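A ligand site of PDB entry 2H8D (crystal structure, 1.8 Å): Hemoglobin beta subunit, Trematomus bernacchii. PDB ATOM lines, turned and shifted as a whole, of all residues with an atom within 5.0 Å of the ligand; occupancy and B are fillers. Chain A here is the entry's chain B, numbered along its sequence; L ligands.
The backbone NH of Leu 96 lies within hydrogen-bond range of the backbone carbonyl oxygen of Leu 91 (3.1 Å). The backbone NH (N) of Val 98 is in hydrogen-bond range of the backbone carbonyl oxygen (O) of His 92 (2.9 Å). O of Phe 103 sits at hydrogen-bond distance from OG of Ser 107 (3.0 Å). O of Leu 71 sits close to OH of Tyr 85 (3.4 Å). The backbone carbonyl oxygen of Leu 88 sits at hydrogen-bond distance from a ring nitrogen (ND1) of His 92 (2.7 Å).
NE2 of His 63 lies close to N4 of the ligand (3.2 Å). Merely in contact with the ligand: Thr 38 (3.3 Å), Val 67 (3.3 Å), Leu 96 (3.3 Å), His 41 (3.4 Å), Phe 42 (3.5 Å), Phe 103 (3.5 Å), Leu 91 (3.6 Å), Leu 141 (3.7 Å), Asn 102 (3.8 Å), Val 98 (3.8 Å), Leu 88 (3.8 Å), Leu 106 (3.9 Å) and Leu 71 (3.9 Å). The nearest printed residue that does not touch the ligand is Gly 70 (4.1 Å).
The side-chain amino group of Lys 66 is in salt-bridge range of an oxygen (O1) of the ligand, at 3.7 Å. An iron atom (FE1) of the ligand is bound by a ring nitrogen (NE2) of His 92 (2.2 Å).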
ATOM      1  N   THR A  38       2.906  17.241   2.137  1.00  0.00           N
ATOM      2  CA  THR A  38       2.008  18.394   1.875  1.00  0.00           C
ATOM      3  C   THR A  38       1.091  18.127   0.703  1.00  0.00           C
ATOM      4  O   THR A  38       0.089  18.816   0.413  1.00  0.00           O
ATOM      5  CB  THR A  38       2.824  19.678   1.666  1.00  0.00           C
ATOM      6  OG1 THR A  38       3.818  19.521   0.648  1.00  0.00           O
ATOM      7  CG2 THR A  38       3.555  19.985   2.969  1.00  0.00           C
ATOM      8  N   HIS A  41      -3.372  17.428   0.359  1.00  0.00           N
ATOM      9  CA  HIS A  41      -4.518  18.239  -0.020  1.00  0.00           C
ATOM     10  C   HIS A  41      -4.804  18.300  -1.494  1.00  0.00           C
ATOM     11  O   HIS A  41      -5.833  18.845  -1.905  1.00  0.00           O
ATOM     12  CB  HIS A  41      -4.232  19.678   0.512  1.00  0.00           C
ATOM     13  CG  HIS A  41      -3.876  19.502   1.970  1.00  0.00           C
ATOM     14  ND1 HIS A  41      -4.864  19.167   2.885  1.00  0.00           N
ATOM     15  CD2 HIS A  41      -2.726  19.567   2.645  1.00  0.00           C
ATOM     16  CE1 HIS A  41      -4.308  19.054   4.082  1.00  0.00           C
ATOM     17  NE2 HIS A  41      -3.008  19.290   3.970  1.00  0.00           N
ATOM     18  N   PHE A  42      -3.909  17.757  -2.324  1.00  0.00           N
ATOM     19  CA  PHE A  42      -4.030  17.957  -3.753  1.00  0.00           C
ATOM     20  C   PHE A  42      -4.293  16.720  -4.574  1.00  0.00           C
ATOM     21  O   PHE A  42      -3.822  16.689  -5.719  1.00  0.00           O
ATOM     22  CB  PHE A  42      -2.715  18.616  -4.205  1.00  0.00           C
ATOM     23  CG  PHE A  42      -2.412  19.871  -3.400  1.00  0.00           C
ATOM     24  CD1 PHE A  42      -3.251  20.990  -3.475  1.00  0.00           C
ATOM     25  CD2 PHE A  42      -1.308  19.965  -2.571  1.00  0.00           C
ATOM     26  CE1 PHE A  42      -2.966  22.126  -2.742  1.00  0.00           C
ATOM     27  CE2 PHE A  42      -1.027  21.104  -1.855  1.00  0.00           C
ATOM     28  CZ  PHE A  42      -1.850  22.205  -1.924  1.00  0.00           C
ATOM     29  N   PHE A  45      -5.605  17.192  -7.965  1.00  0.00           N
ATOM     30  CA  PHE A  45      -4.760  17.983  -8.871  1.00  0.00           C
ATOM     31  C   PHE A  45      -4.184  17.148  -9.995  1.00  0.00           C
ATOM     32  O   PHE A  45      -3.502  17.648 -10.890  1.00  0.00           O
ATOM     33  CB  PHE A  45      -3.641  18.636  -8.035  1.00  0.00           C
ATOM     34  CG  PHE A  45      -4.170  19.931  -7.405  1.00  0.00           C
ATOM     35  CD1 PHE A  45      -5.377  19.915  -6.730  1.00  0.00           C
ATOM     36  CD2 PHE A  45      -3.465  21.112  -7.509  1.00  0.00           C
ATOM     37  CE1 PHE A  45      -5.865  21.081  -6.160  1.00  0.00           C
ATOM     38  CE2 PHE A  45      -3.954  22.287  -6.944  1.00  0.00           C
ATOM     39  CZ  PHE A  45      -5.164  22.274  -6.285  1.00  0.00           C
ATOM     40  N   HIS A  63      -2.275  26.823  -8.541  1.00  0.00           N
ATOM     41  CA  HIS A  63      -2.431  26.968  -7.097  1.00  0.00           C
ATOM     42  C   HIS A  63      -1.221  27.667  -6.493  1.00  0.00           C
ATOM     43  O   HIS A  63      -1.422  28.416  -5.531  1.00  0.00           O
ATOM     44  CB  HIS A  63      -2.611  25.632  -6.375  1.00  0.00           C
ATOM     45  CG  HIS A  63      -3.210  25.855  -5.011  1.00  0.00           C
ATOM     46  ND1 HIS A  63      -4.514  26.263  -4.876  1.00  0.00           N
ATOM     47  CD2 HIS A  63      -2.723  25.732  -3.756  1.00  0.00           C
ATOM     48  CE1 HIS A  63      -4.811  26.383  -3.589  1.00  0.00           C
ATOM     49  NE2 HIS A  63      -3.743  26.067  -2.893  1.00  0.00           N
ATOM     50  N   LYS A  66      -1.693  31.384  -6.843  1.00  0.00           N
ATOM     51  CA  LYS A  66      -2.746  31.803  -5.921  1.00  0.00           C
ATOM     52  C   LYS A  66      -2.239  31.950  -4.497  1.00  0.00           C
ATOM     53  O   LYS A  66      -2.468  32.959  -3.838  1.00  0.00           O
ATOM     54  CB  LYS A  66      -3.929  30.811  -5.937  1.00  0.00           C
ATOM     55  CG  LYS A  66      -5.111  31.310  -5.102  1.00  0.00           C
ATOM     56  CD  LYS A  66      -6.392  31.071  -5.873  1.00  0.00           C
ATOM     57  CE  LYS A  66      -6.606  29.614  -6.189  1.00  0.00           C
ATOM     58  NZ  LYS A  66      -8.047  29.192  -6.109  1.00  0.00           N
ATOM     59  N   VAL A  67      -1.557  30.932  -3.981  1.00  0.00           N
ATOM     60  CA  VAL A  67      -1.000  31.037  -2.647  1.00  0.00           C
ATOM     61  C   VAL A  67      -0.084  32.248  -2.510  1.00  0.00           C
ATOM     62  O   VAL A  67      -0.121  32.974  -1.514  1.00  0.00           O
ATOM     63  CB  VAL A  67      -0.189  29.783  -2.261  1.00  0.00           C
ATOM     64  CG1 VAL A  67       0.598  30.082  -1.004  1.00  0.00           C
ATOM     65  CG2 VAL A  67      -1.141  28.614  -2.091  1.00  0.00           C
ATOM     66  N   GLY A  70      -1.847  35.279  -2.268  1.00  0.00           N
ATOM     67  CA  GLY A  70      -2.414  35.369  -0.928  1.00  0.00           C
ATOM     68  C   GLY A  70      -1.553  36.171   0.001  1.00  0.00           C
ATOM     69  O   GLY A  70      -1.941  36.641   1.086  1.00  0.00           O
ATOM     70  N   LEU A  71      -0.282  36.414  -0.288  1.00  0.00           N
ATOM     71  CA  LEU A  71       0.510  37.218   0.611  1.00  0.00           C
ATOM     72  C   LEU A  71       0.238  38.715   0.364  1.00  0.00           C
ATOM     73  O   LEU A  71       0.606  39.501   1.213  1.00  0.00           O
ATOM     74  CB  LEU A  71       2.027  37.005   0.468  1.00  0.00           C
ATOM     75  CG  LEU A  71       2.514  35.546   0.490  1.00  0.00           C
ATOM     76  CD1 LEU A  71       4.001  35.463   0.168  1.00  0.00           C
ATOM     77  CD2 LEU A  71       2.207  34.920   1.843  1.00  0.00           C
ATOM     78  N   ARG A  73      -2.430  40.644   0.417  1.00  0.00           N
ATOM     79  CA  ARG A  73      -3.205  41.329   1.459  1.00  0.00           C
ATOM     80  C   ARG A  73      -2.372  41.628   2.684  1.00  0.00           C
ATOM     81  O   ARG A  73      -2.636  42.606   3.398  1.00  0.00           O
ATOM     82  CB  ARG A  73      -4.433  40.530   1.866  1.00  0.00           C
ATOM     83  CG  ARG A  73      -4.130  39.235   2.608  1.00  0.00           C
ATOM     84  CD  ARG A  73      -5.320  38.291   2.553  1.00  0.00           C
ATOM     85  NE  ARG A  73      -5.616  37.843   1.189  1.00  0.00           N
ATOM     86  CZ  ARG A  73      -6.730  37.183   0.905  1.00  0.00           C
ATOM     87  NH1 ARG A  73      -7.584  36.954   1.895  1.00  0.00           N
ATOM     88  NH2 ARG A  73      -7.001  36.781  -0.309  1.00  0.00           N
ATOM     89  N   TYR A  85      -6.025  37.940   7.918  1.00  0.00           N
ATOM     90  CA  TYR A  85      -6.013  36.541   7.501  1.00  0.00           C
ATOM     91  C   TYR A  85      -6.994  35.664   8.241  1.00  0.00           C
ATOM     92  O   TYR A  85      -7.038  34.466   7.961  1.00  0.00           O
ATOM     93  CB  TYR A  85      -4.561  36.026   7.658  1.00  0.00           C
ATOM     94  CG  TYR A  85      -3.695  36.508   6.523  1.00  0.00           C
ATOM     95  CD1 TYR A  85      -3.719  35.777   5.330  1.00  0.00           C
ATOM     96  CD2 TYR A  85      -2.886  37.629   6.613  1.00  0.00           C
ATOM     97  CE1 TYR A  85      -2.939  36.184   4.282  1.00  0.00           C
ATOM     98  CE2 TYR A  85      -2.095  38.039   5.546  1.00  0.00           C
ATOM     99  CZ  TYR A  85      -2.142  37.303   4.391  1.00  0.00           C
ATOM    100  OH  TYR A  85      -1.402  37.637   3.275  1.00  0.00           O
ATOM    101  N   LEU A  88      -9.133  33.400   5.984  1.00  0.00           N
ATOM    102  CA  LEU A  88      -8.302  32.395   5.321  1.00  0.00           C
ATOM    103  C   LEU A  88      -7.889  31.274   6.293  1.00  0.00           C
ATOM    104  O   LEU A  88      -7.846  30.101   5.937  1.00  0.00           O
ATOM    105  CB  LEU A  88      -7.040  33.041   4.763  1.00  0.00           C
ATOM    106  CG  LEU A  88      -6.535  32.636   3.391  1.00  0.00           C
ATOM    107  CD1 LEU A  88      -7.657  32.211   2.450  1.00  0.00           C
ATOM    108  CD2 LEU A  88      -5.748  33.781   2.743  1.00  0.00           C
ATOM    109  N   LEU A  91     -10.715  29.136   6.912  1.00  0.00           N
ATOM    110  CA  LEU A  91     -10.894  28.308   5.731  1.00  0.00           C
ATOM    111  C   LEU A  91      -9.981  27.080   5.779  1.00  0.00           C
ATOM    112  O   LEU A  91     -10.428  25.935   5.627  1.00  0.00           O
ATOM    113  CB  LEU A  91     -10.610  29.124   4.466  1.00  0.00           C
ATOM    114  CG  LEU A  91     -10.510  28.341   3.151  1.00  0.00           C
ATOM    115  CD1 LEU A  91     -11.879  28.225   2.499  1.00  0.00           C
ATOM    116  CD2 LEU A  91      -9.501  28.962   2.195  1.00  0.00           C
ATOM    117  N   HIS A  92      -8.692  27.326   5.995  1.00  0.00           N
ATOM    118  CA  HIS A  92      -7.708  26.239   5.998  1.00  0.00           C
ATOM    119  C   HIS A  92      -7.944  25.251   7.119  1.00  0.00           C
ATOM    120  O   HIS A  92      -7.739  24.046   7.004  1.00  0.00           O
ATOM    121  CB  HIS A  92      -6.310  26.871   6.048  1.00  0.00           C
ATOM    122  CG  HIS A  92      -5.857  27.409   4.717  1.00  0.00           C
ATOM    123  ND1 HIS A  92      -6.214  28.666   4.262  1.00  0.00           N
ATOM    124  CD2 HIS A  92      -5.087  26.864   3.731  1.00  0.00           C
ATOM    125  CE1 HIS A  92      -5.687  28.875   3.070  1.00  0.00           C
ATOM    126  NE2 HIS A  92      -5.003  27.790   2.733  1.00  0.00           N
ATOM    127  N   LEU A  96     -10.608  22.924   4.722  1.00  0.00           N
ATOM    128  CA  LEU A  96      -9.531  22.270   3.995  1.00  0.00           C
ATOM    129  C   LEU A  96      -8.766  21.296   4.887  1.00  0.00           C
ATOM    130  O   LEU A  96      -8.108  20.398   4.349  1.00  0.00           O
ATOM    131  CB  LEU A  96      -8.552  23.298   3.418  1.00  0.00           C
ATOM    132  CG  LEU A  96      -9.156  24.344   2.461  1.00  0.00           C
ATOM    133  CD1 LEU A  96      -8.151  25.436   2.177  1.00  0.00           C
ATOM    134  CD2 LEU A  96      -9.648  23.722   1.165  1.00  0.00           C
ATOM    135  N   VAL A  98      -6.051  21.704   6.490  1.00  0.00           N
ATOM    136  CA  VAL A  98      -4.620  21.742   6.258  1.00  0.00           C
ATOM    137  C   VAL A  98      -3.828  21.874   7.539  1.00  0.00           C
ATOM    138  O   VAL A  98      -4.033  22.780   8.345  1.00  0.00           O
ATOM    139  CB  VAL A  98      -4.245  22.929   5.325  1.00  0.00           C
ATOM    140  CG1 VAL A  98      -2.735  23.133   5.357  1.00  0.00           C
ATOM    141  CG2 VAL A  98      -4.772  22.662   3.911  1.00  0.00           C
ATOM    142  N   ASN A 102       2.446  22.860   7.740  1.00  0.00           N
ATOM    143  CA  ASN A 102       2.754  22.846   6.306  1.00  0.00           C
ATOM    144  C   ASN A 102       3.005  24.287   5.840  1.00  0.00           C
ATOM    145  O   ASN A 102       3.800  24.539   4.929  1.00  0.00           O
ATOM    146  CB  ASN A 102       1.638  22.215   5.489  1.00  0.00           C
ATOM    147  CG  ASN A 102       1.431  20.712   5.609  1.00  0.00           C
ATOM    148  OD1 ASN A 102       0.466  20.163   5.056  1.00  0.00           O
ATOM    149  ND2 ASN A 102       2.301  20.012   6.315  1.00  0.00           N
ATOM    150  N   PHE A 103       2.323  25.253   6.450  1.00  0.00           N
ATOM    151  CA  PHE A 103       2.582  26.644   6.083  1.00  0.00           C
ATOM    152  C   PHE A 103       4.054  27.006   6.231  1.00  0.00           C
ATOM    153  O   PHE A 103       4.653  27.710   5.395  1.00  0.00           O
ATOM    154  CB  PHE A 103       1.747  27.610   6.937  1.00  0.00           C
ATOM    155  CG  PHE A 103       0.248  27.419   6.839  1.00  0.00           C
ATOM    156  CD1 PHE A 103      -0.409  27.113   5.678  1.00  0.00           C
ATOM    157  CD2 PHE A 103      -0.555  27.549   7.970  1.00  0.00           C
ATOM    158  CE1 PHE A 103      -1.776  26.942   5.556  1.00  0.00           C
ATOM    159  CE2 PHE A 103      -1.922  27.369   7.894  1.00  0.00           C
ATOM    160  CZ  PHE A 103      -2.561  27.061   6.706  1.00  0.00           C
ATOM    161  N   LEU A 106       6.079  25.492   3.329  1.00  0.00           N
ATOM    162  CA  LEU A 106       5.886  26.229   2.080  1.00  0.00           C
ATOM    163  C   LEU A 106       6.664  27.534   2.158  1.00  0.00           C
ATOM    164  O   LEU A 106       7.320  27.857   1.143  1.00  0.00           O
ATOM    165  CB  LEU A 106       4.407  26.503   1.765  1.00  0.00           C
ATOM    166  CG  LEU A 106       4.193  27.216   0.427  1.00  0.00           C
ATOM    167  CD1 LEU A 106       4.867  26.430  -0.706  1.00  0.00           C
ATOM    168  CD2 LEU A 106       2.721  27.443   0.152  1.00  0.00           C
ATOM    169  N   SER A 107       6.581  28.190   3.312  1.00  0.00           N
ATOM    170  CA  SER A 107       7.285  29.460   3.469  1.00  0.00           C
ATOM    171  C   SER A 107       8.769  29.364   3.163  1.00  0.00           C
ATOM    172  O   SER A 107       9.375  30.205   2.504  1.00  0.00           O
ATOM    173  CB  SER A 107       7.165  30.005   4.914  1.00  0.00           C
ATOM    174  OG  SER A 107       5.837  30.459   5.077  1.00  0.00           O
ATOM    175  N   ILE A 110       9.352  28.993  -0.562  1.00  0.00           N
ATOM    176  CA  ILE A 110       9.228  30.340  -1.167  1.00  0.00           C
ATOM    177  C   ILE A 110      10.485  31.125  -0.973  1.00  0.00           C
ATOM    178  O   ILE A 110      11.111  31.724  -1.863  1.00  0.00           O
ATOM    179  CB  ILE A 110       8.012  31.089  -0.540  1.00  0.00           C
ATOM    180  CG1 ILE A 110       6.716  30.335  -0.711  1.00  0.00           C
ATOM    181  CG2 ILE A 110       7.974  32.499  -1.103  1.00  0.00           C
ATOM    182  CD1 ILE A 110       5.447  31.004  -0.186  1.00  0.00           C
ATOM    183  N   VAL A 137       2.762  36.165   8.775  1.00  0.00           N
ATOM    184  CA  VAL A 137       1.668  35.661   7.961  1.00  0.00           C
ATOM    185  C   VAL A 137       1.324  34.236   8.385  1.00  0.00           C
ATOM    186  O   VAL A 137       0.159  33.870   8.528  1.00  0.00           O
ATOM    187  CB  VAL A 137       2.037  35.720   6.461  1.00  0.00           C
ATOM    188  CG1 VAL A 137       1.007  35.006   5.602  1.00  0.00           C
ATOM    189  CG2 VAL A 137       2.212  37.188   6.018  1.00  0.00           C
ATOM    190  N   LEU A 141      -2.163  32.702   9.738  1.00  0.00           N
ATOM    191  CA  LEU A 141      -2.869  31.599   9.097  1.00  0.00           C
ATOM    192  C   LEU A 141      -3.159  30.459  10.065  1.00  0.00           C
ATOM    193  O   LEU A 141      -4.135  29.736   9.921  1.00  0.00           O
ATOM    194  CB  LEU A 141      -2.040  31.110   7.902  1.00  0.00           C
ATOM    195  CG  LEU A 141      -2.114  31.942   6.640  1.00  0.00           C
ATOM    196  CD1 LEU A 141      -0.985  31.579   5.660  1.00  0.00           C
ATOM    197  CD2 LEU A 141      -3.460  31.764   5.952  1.00  0.00           C
HETATM  198  C1  LIG L   1      -6.606  27.772  -0.990  1.00  0.00           C
HETATM  199  C2  LIG L   1      -3.494  31.070   0.656  1.00  0.00           C
HETATM  200  C3  LIG L   1      -0.557  27.538   2.177  1.00  0.00           C
HETATM  201  C4  LIG L   1      -3.697  24.262   0.621  1.00  0.00           C
HETATM  202  C5  LIG L   1      -6.109  29.000  -0.575  1.00  0.00           C
HETATM  203  C6  LIG L   1      -6.484  30.290  -1.140  1.00  0.00           C
HETATM  204  C7  LIG L   1      -5.630  31.204  -0.649  1.00  0.00           C
HETATM  205  C8  LIG L   1      -4.527  30.468  -0.052  1.00  0.00           C
HETATM  206  C9  LIG L   1      -5.572  32.720  -0.937  1.00  0.00           C
HETATM  207  C10 LIG L   1      -7.800  30.550  -1.903  1.00  0.00           C
HETATM  208  C11 LIG L   1      -9.094  30.433  -1.103  1.00  0.00           C
HETATM  209  C12 LIG L   1     -10.280  29.924  -1.868  1.00  0.00           C
HETATM  210  O1  LIG L   1     -10.157  29.840  -3.122  1.00  0.00           O
HETATM  211  O2  LIG L   1     -11.302  29.602  -1.205  1.00  0.00           O
HETATM  212  C13 LIG L   1      -2.413  30.398   1.207  1.00  0.00           C
HETATM  213  C14 LIG L   1      -1.238  31.020   1.776  1.00  0.00           C
HETATM  214  C15 LIG L   1      -0.410  30.037   2.138  1.00  0.00           C
HETATM  215  C16 LIG L   1      -1.151  28.786   2.025  1.00  0.00           C
HETATM  216  C17 LIG L   1      -1.086  32.544   1.970  1.00  0.00           C
HETATM  217  C18 LIG L   1       0.960  30.101   2.841  1.00  0.00           C
HETATM  218  C19 LIG L   1       1.779  31.132   2.734  1.00  0.00           C
HETATM  219  C20 LIG L   1      -1.207  26.333   2.050  1.00  0.00           C
HETATM  220  C21 LIG L   1      -0.541  25.030   2.081  1.00  0.00           C
HETATM  221  C22 LIG L   1      -1.410  24.122   1.671  1.00  0.00           C
HETATM  222  C23 LIG L   1      -2.559  24.833   1.142  1.00  0.00           C
HETATM  223  C24 LIG L   1       0.931  24.870   2.531  1.00  0.00           C
HETATM  224  C25 LIG L   1      -1.362  22.576   1.730  1.00  0.00           C
HETATM  225  C26 LIG L   1      -0.237  21.927   1.421  1.00  0.00           C
HETATM  226  C27 LIG L   1      -4.700  24.941  -0.060  1.00  0.00           C
HETATM  227  C28 LIG L   1      -5.903  24.308  -0.538  1.00  0.00           C
HETATM  228  C29 LIG L   1      -6.790  25.267  -0.828  1.00  0.00           C
HETATM  229  C30 LIG L   1      -6.150  26.531  -0.584  1.00  0.00           C
HETATM  230  C31 LIG L   1      -6.125  22.770  -0.551  1.00  0.00           C
HETATM  231  C32 LIG L   1      -8.043  25.074  -1.733  1.00  0.00           C
HETATM  232  C33 LIG L   1      -7.730  24.679  -3.184  1.00  0.00           C
HETATM  233  C34 LIG L   1      -8.911  24.461  -4.088  1.00  0.00           C
HETATM  234  O3  LIG L   1      -8.932  25.123  -5.163  1.00  0.00           O
HETATM  235  O4  LIG L   1      -9.789  23.644  -3.729  1.00  0.00           O
HETATM  236  N1  LIG L   1      -4.914  29.153   0.111  1.00  0.00           N
HETATM  237  N2  LIG L   1      -2.354  29.024   1.377  1.00  0.00           N
HETATM  238  N3  LIG L   1      -2.456  26.175   1.473  1.00  0.00           N
HETATM  239  N4  LIG L   1      -4.926  26.314   0.058  1.00  0.00           N
HETATM  240 FE1  LIG L   1      -3.682  27.657   0.920  1.00  0.00          FE
